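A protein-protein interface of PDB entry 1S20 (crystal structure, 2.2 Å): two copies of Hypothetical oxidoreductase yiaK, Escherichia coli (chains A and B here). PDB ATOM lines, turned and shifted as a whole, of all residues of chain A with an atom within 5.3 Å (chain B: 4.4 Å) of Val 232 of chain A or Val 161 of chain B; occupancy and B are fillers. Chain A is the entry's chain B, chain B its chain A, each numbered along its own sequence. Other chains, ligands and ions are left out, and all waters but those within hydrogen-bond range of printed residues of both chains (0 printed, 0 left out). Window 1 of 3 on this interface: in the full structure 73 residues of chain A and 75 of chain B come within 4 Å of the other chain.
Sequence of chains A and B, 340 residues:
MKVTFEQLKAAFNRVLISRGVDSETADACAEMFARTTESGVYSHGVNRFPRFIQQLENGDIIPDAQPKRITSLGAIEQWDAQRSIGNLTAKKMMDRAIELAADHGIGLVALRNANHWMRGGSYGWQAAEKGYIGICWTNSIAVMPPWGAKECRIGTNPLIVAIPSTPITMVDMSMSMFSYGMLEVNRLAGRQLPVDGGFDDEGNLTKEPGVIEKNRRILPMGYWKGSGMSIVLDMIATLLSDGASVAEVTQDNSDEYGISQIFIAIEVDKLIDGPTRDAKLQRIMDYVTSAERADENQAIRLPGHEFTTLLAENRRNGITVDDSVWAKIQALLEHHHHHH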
ATOM      1  N   GLY A 228       4.519 -16.434   4.826  1.00  0.00           N
ATOM      2  CA  GLY A 228       5.785 -16.697   5.481  1.00  0.00           C
ATOM      3  C   GLY A 228       5.638 -17.538   6.742  1.00  0.00           C
ATOM      4  O   GLY A 228       6.401 -18.479   6.957  1.00  0.00           O
ATOM      5  N   MET A 229       4.664 -17.205   7.585  1.00  0.00           N
ATOM      6  CA  MET A 229       4.450 -17.954   8.819  1.00  0.00           C
ATOM      7  C   MET A 229       4.109 -19.393   8.487  1.00  0.00           C
ATOM      8  O   MET A 229       4.573 -20.314   9.148  1.00  0.00           O
ATOM      9  CB  MET A 229       3.320 -17.334   9.653  1.00  0.00           C
ATOM     10  CG  MET A 229       3.776 -16.253  10.626  1.00  0.00           C
ATOM     11  SD  MET A 229       4.944 -16.973  12.005  1.00  0.00           S
ATOM     12  CE  MET A 229       3.581 -17.537  13.262  1.00  0.00           C
ATOM     13  N   SER A 230       3.306 -19.597   7.454  1.00  0.00           N
ATOM     14  CA  SER A 230       2.951 -20.958   7.078  1.00  0.00           C
ATOM     15  C   SER A 230       4.180 -21.801   6.772  1.00  0.00           C
ATOM     16  O   SER A 230       4.305 -22.934   7.237  1.00  0.00           O
ATOM     17  CB  SER A 230       2.054 -20.967   5.851  1.00  0.00           C
ATOM     18  OG  SER A 230       1.916 -22.298   5.395  1.00  0.00           O
ATOM     19  N   ILE A 231       5.086 -21.238   5.979  1.00  0.00           N
ATOM     20  CA  ILE A 231       6.293 -21.947   5.599  1.00  0.00           C
ATOM     21  C   ILE A 231       7.186 -22.257   6.796  1.00  0.00           C
ATOM     22  O   ILE A 231       7.649 -23.397   6.928  1.00  0.00           O
ATOM     23  CB  ILE A 231       7.076 -21.159   4.523  1.00  0.00           C
ATOM     24  CG1 ILE A 231       6.189 -20.957   3.299  1.00  0.00           C
ATOM     25  CG2 ILE A 231       8.312 -21.929   4.088  1.00  0.00           C
ATOM     26  CD1 ILE A 231       6.822 -20.105   2.222  1.00  0.00           C
ATOM     27  N   VAL A 232       7.411 -21.277   7.679  1.00  0.00           N
ATOM     28  CA  VAL A 232       8.276 -21.522   8.837  1.00  0.00           C
ATOM     29  C   VAL A 232       7.670 -22.548   9.780  1.00  0.00           C
ATOM     30  O   VAL A 232       8.395 -23.314  10.403  1.00  0.00           O
ATOM     31  CB  VAL A 232       8.600 -20.239   9.680  1.00  0.00           C
ATOM     32  CG1 VAL A 232       9.376 -19.242   8.835  1.00  0.00           C
ATOM     33  CG2 VAL A 232       7.325 -19.615  10.252  1.00  0.00           C
ATOM     34  N   LEU A 233       6.347 -22.563   9.894  1.00  0.00           N
ATOM     35  CA  LEU A 233       5.687 -23.522  10.776  1.00  0.00           C
ATOM     36  C   LEU A 233       5.797 -24.925  10.178  1.00  0.00           C
ATOM     37  O   LEU A 233       5.831 -25.911  10.907  1.00  0.00           O
ATOM     38  CB  LEU A 233       4.217 -23.134  10.971  1.00  0.00           C
ATOM     39  CG  LEU A 233       3.948 -21.826  11.723  1.00  0.00           C
ATOM     40  CD1 LEU A 233       2.448 -21.602  11.826  1.00  0.00           C
ATOM     41  CD2 LEU A 233       4.576 -21.881  13.120  1.00  0.00           C
ATOM     42  N   ASP A 234       5.845 -25.006   8.850  1.00  0.00           N
ATOM     43  CA  ASP A 234       5.968 -26.288   8.142  1.00  0.00           C
ATOM     44  C   ASP A 234       7.382 -26.820   8.382  1.00  0.00           C
ATOM     45  O   ASP A 234       7.558 -27.985   8.728  1.00  0.00           O
ATOM     46  CB  ASP A 234       5.692 -26.072   6.640  1.00  0.00           C
ATOM     47  CG  ASP A 234       5.845 -27.344   5.792  1.00  0.00           C
ATOM     48  OD1 ASP A 234       5.437 -28.449   6.207  1.00  0.00           O
ATOM     49  OD2 ASP A 234       6.369 -27.227   4.669  1.00  0.00           O
ATOM     50  N   MET A 235       8.380 -25.957   8.225  1.00  0.00           N
ATOM     51  CA  MET A 235       9.762 -26.364   8.432  1.00  0.00           C
ATOM     52  C   MET A 235       9.996 -26.872   9.852  1.00  0.00           C
ATOM     53  O   MET A 235      10.618 -27.916  10.032  1.00  0.00           O
ATOM     54  CB  MET A 235      10.718 -25.201   8.152  1.00  0.00           C
ATOM     55  CG  MET A 235      10.646 -24.663   6.734  1.00  0.00           C
ATOM     56  SD  MET A 235      11.841 -23.183   6.512  1.00  0.00           S
ATOM     57  CE  MET A 235      12.536 -23.665   4.817  1.00  0.00           C
ATOM     58  N   ILE A 236       9.494 -26.138  10.848  1.00  0.00           N
ATOM     59  CA  ILE A 236       9.651 -26.539  12.245  1.00  0.00           C
ATOM     60  C   ILE A 236       8.956 -27.869  12.536  1.00  0.00           C
ATOM     61  O   ILE A 236       9.518 -28.727  13.218  1.00  0.00           O
ATOM     62  CB  ILE A 236       9.082 -25.492  13.234  1.00  0.00           C
ATOM     63  CG1 ILE A 236       9.774 -24.139  13.039  1.00  0.00           C
ATOM     64  CG2 ILE A 236       9.276 -25.996  14.673  1.00  0.00           C
ATOM     65  CD1 ILE A 236       9.226 -23.014  13.908  1.00  0.00           C
ATOM     66  N   ALA A 237       7.728 -28.034  12.049  1.00  0.00           N
ATOM     67  CA  ALA A 237       7.004 -29.283  12.279  1.00  0.00           C
ATOM     68  C   ALA A 237       7.706 -30.435  11.558  1.00  0.00           C
ATOM     69  O   ALA A 237       7.749 -31.549  12.062  1.00  0.00           O
ATOM     70  CB  ALA A 237       5.568 -29.162  11.797  1.00  0.00           C
ATOM     71  N   GLY B 134      15.054 -20.401  15.930  1.00  0.00           N
ATOM     72  CA  GLY B 134      14.933 -19.219  16.753  1.00  0.00           C
ATOM     73  C   GLY B 134      13.548 -18.602  16.736  1.00  0.00           C
ATOM     74  O   GLY B 134      13.008 -18.272  15.680  1.00  0.00           O
ATOM     75  N   ILE B 135      12.977 -18.449  17.925  1.00  0.00           N
ATOM     76  CA  ILE B 135      11.658 -17.859  18.079  1.00  0.00           C
ATOM     77  C   ILE B 135      11.721 -16.878  19.240  1.00  0.00           C
ATOM     78  O   ILE B 135      12.216 -17.214  20.321  1.00  0.00           O
ATOM     79  CB  ILE B 135      10.602 -18.934  18.379  1.00  0.00           C
ATOM     80  CG1 ILE B 135      10.488 -19.883  17.193  1.00  0.00           C
ATOM     81  CG2 ILE B 135       9.255 -18.291  18.689  1.00  0.00           C
ATOM     82  CD1 ILE B 135       9.787 -21.171  17.524  1.00  0.00           C
ATOM     83  N   LEU B 159       6.733 -10.890  16.176  1.00  0.00           N
ATOM     84  CA  LEU B 159       7.039 -12.302  16.341  1.00  0.00           C
ATOM     85  C   LEU B 159       8.133 -12.668  15.344  1.00  0.00           C
ATOM     86  O   LEU B 159       7.997 -12.434  14.141  1.00  0.00           O
ATOM     87  CB  LEU B 159       5.780 -13.144  16.098  1.00  0.00           C
ATOM     88  CG  LEU B 159       5.921 -14.670  16.107  1.00  0.00           C
ATOM     89  CD1 LEU B 159       6.530 -15.137  17.418  1.00  0.00           C
ATOM     90  CD2 LEU B 159       4.554 -15.301  15.887  1.00  0.00           C
ATOM     91  N   ILE B 160       9.226 -13.219  15.859  1.00  0.00           N
ATOM     92  CA  ILE B 160      10.364 -13.632  15.040  1.00  0.00           C
ATOM     93  C   ILE B 160      10.482 -15.163  15.090  1.00  0.00           C
ATOM     94  O   ILE B 160      10.448 -15.757  16.173  1.00  0.00           O
ATOM     95  CB  ILE B 160      11.696 -12.996  15.561  1.00  0.00           C
ATOM     96  CG1 ILE B 160      11.750 -11.496  15.237  1.00  0.00           C
ATOM     97  CG2 ILE B 160      12.894 -13.703  14.937  1.00  0.00           C
ATOM     98  CD1 ILE B 160      10.764 -10.607  16.015  1.00  0.00           C
ATOM     99  N   VAL B 161      10.601 -15.782  13.913  1.00  0.00           N
ATOM    100  CA  VAL B 161      10.730 -17.237  13.756  1.00  0.00           C
ATOM    101  C   VAL B 161      11.782 -17.473  12.671  1.00  0.00           C
ATOM    102  O   VAL B 161      11.533 -17.192  11.497  1.00  0.00           O
ATOM    103  CB  VAL B 161       9.403 -17.900  13.278  1.00  0.00           C
ATOM    104  CG1 VAL B 161       9.594 -19.399  13.112  1.00  0.00           C
ATOM    105  CG2 VAL B 161       8.282 -17.612  14.248  1.00  0.00           C
ATOM    106  N   ALA B 162      12.950 -17.977  13.069  1.00  0.00           N
ATOM    107  CA  ALA B 162      14.051 -18.243  12.144  1.00  0.00           C
ATOM    108  C   ALA B 162      14.413 -19.726  12.122  1.00  0.00           C
ATOM    109  O   ALA B 162      14.491 -20.371  13.164  1.00  0.00           O
ATOM    110  CB  ALA B 162      15.275 -17.411  12.534  1.00  0.00           C
ATOM    111  N   ILE B 163      14.639 -20.242  10.916  1.00  0.00           N
ATOM    112  CA  ILE B 163      14.971 -21.639  10.680  1.00  0.00           C
ATOM    113  C   ILE B 163      16.419 -21.745  10.203  1.00  0.00           C
ATOM    114  O   ILE B 163      16.862 -20.968   9.348  1.00  0.00           O
ATOM    115  CB  ILE B 163      14.040 -22.221   9.594  1.00  0.00           C
ATOM    116  CG1 ILE B 163      12.588 -21.830   9.894  1.00  0.00           C
ATOM    117  CG2 ILE B 163      14.203 -23.741   9.497  1.00  0.00           C
ATOM    118  CD1 ILE B 163      12.036 -22.376  11.196  1.00  0.00           C
ATOM    119  N   THR B 169      15.836 -19.056   6.813  1.00  0.00           N
ATOM    120  CA  THR B 169      14.472 -18.624   6.549  1.00  0.00           C
ATOM    121  C   THR B 169      13.916 -18.039   7.841  1.00  0.00           C
ATOM    122  O   THR B 169      13.907 -18.697   8.878  1.00  0.00           O
ATOM    123  CB  THR B 169      13.620 -19.804   6.059  1.00  0.00           C
ATOM    124  OG1 THR B 169      14.143 -20.268   4.807  1.00  0.00           O
ATOM    125  CG2 THR B 169      12.171 -19.385   5.862  1.00  0.00           C
ATOM    126  N   MET B 170      13.457 -16.793   7.773  1.00  0.00           N
ATOM    127  CA  MET B 170      12.965 -16.115   8.963  1.00  0.00           C
ATOM    128  C   MET B 170      11.847 -15.105   8.716  1.00  0.00           C
ATOM    129  O   MET B 170      11.856 -14.370   7.735  1.00  0.00           O
ATOM    130  CB  MET B 170      14.146 -15.411   9.649  1.00  0.00           C
ATOM    131  CG  MET B 170      13.761 -14.542  10.817  1.00  0.00           C
ATOM    132  SD  MET B 170      15.276 -13.748  11.703  1.00  0.00           S
ATOM    133  CE  MET B 170      15.589 -12.219  10.589  1.00  0.00           C
ATOM    134  N   VAL B 171      10.884 -15.071   9.626  1.00  0.00           N
ATOM    135  CA  VAL B 171       9.783 -14.130   9.530  1.00  0.00           C
ATOM    136  C   VAL B 171       9.945 -13.165  10.695  1.00  0.00           C
ATOM    137  O   VAL B 171       9.870 -13.572  11.842  1.00  0.00           O
ATOM    138  CB  VAL B 171       8.429 -14.841   9.668  1.00  0.00           C
ATOM    139  CG1 VAL B 171       8.059 -15.537   8.350  1.00  0.00           C
ATOM    140  CG2 VAL B 171       8.519 -15.865  10.771  1.00  0.00           C
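O of Val 161 of chain B sits at hydrogen-bond distance from N of Val 171 of chain B (2.9 Å). The backbone carbonyl oxygen (O) of Thr 169 of chain B sits at hydrogen-bond distance from the backbone NH (N) of Ile 163 of chain B, at 2.7 Å.
Of the 10 printed residues of chain B, 5 touch a printed residue of chain A. Hydrophobic or aromatic side chains of chain A within 4 Å of the printed part of chain B: Met 229, Val 232, Met 235 and Ile 236. Among the printed residues, 10 pairs touch across the chains.
C of Gly 228 of chain A touches CG1 of Val 171 of chain B, 3.5 Å away. CE of Met 229 of chain A touches CD2 of Leu 159 of chain B, 3.6 Å away. Met 229 of chain A touches Val 171 of chain B. CG1 of Val 161 of chain B touches CG2 of Val 232 of chain A, at 3.7 Å. Val 232 of chain A touches Ile 163 of chain B. Val 171 of chain B touches Val 232 of chain A. Met 235 of chain A touches Ile 163 of chain B (SD to CG1, 3.7 Å). Thr 169 of chain B touches Met 235 of chain A. Ile 236 of chain A touches Val 161 of chain B. CG1 of Ile 236 of chain A touches CD1 of Ile 163 of chain B, at 3.4 Å.
No position is printed for both chains.
Val 232 of chain A touches three residues of chain B. Val 161 of chain B touches two residues of chain A. Of the printed residues of chain B, Met 229 of chain A touches Leu 159 and Val 171. Of the printed residues of chain A, Thr 169 of chain B touches Met 235 (3.8 Å). Printed residues of chain B within 4 Å of Met 235 of chain A: Ile 163 and Thr 169. Gly 134 of chain B touches none of the printed residues of chain A. The nearest residue of chain B that does not touch Val 232 of chain A is Thr 169 of chain B (4.1 Å). The nearest residue of chain A that does not touch Val 161 of chain B is Met 229 of chain A (4.1 Å).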
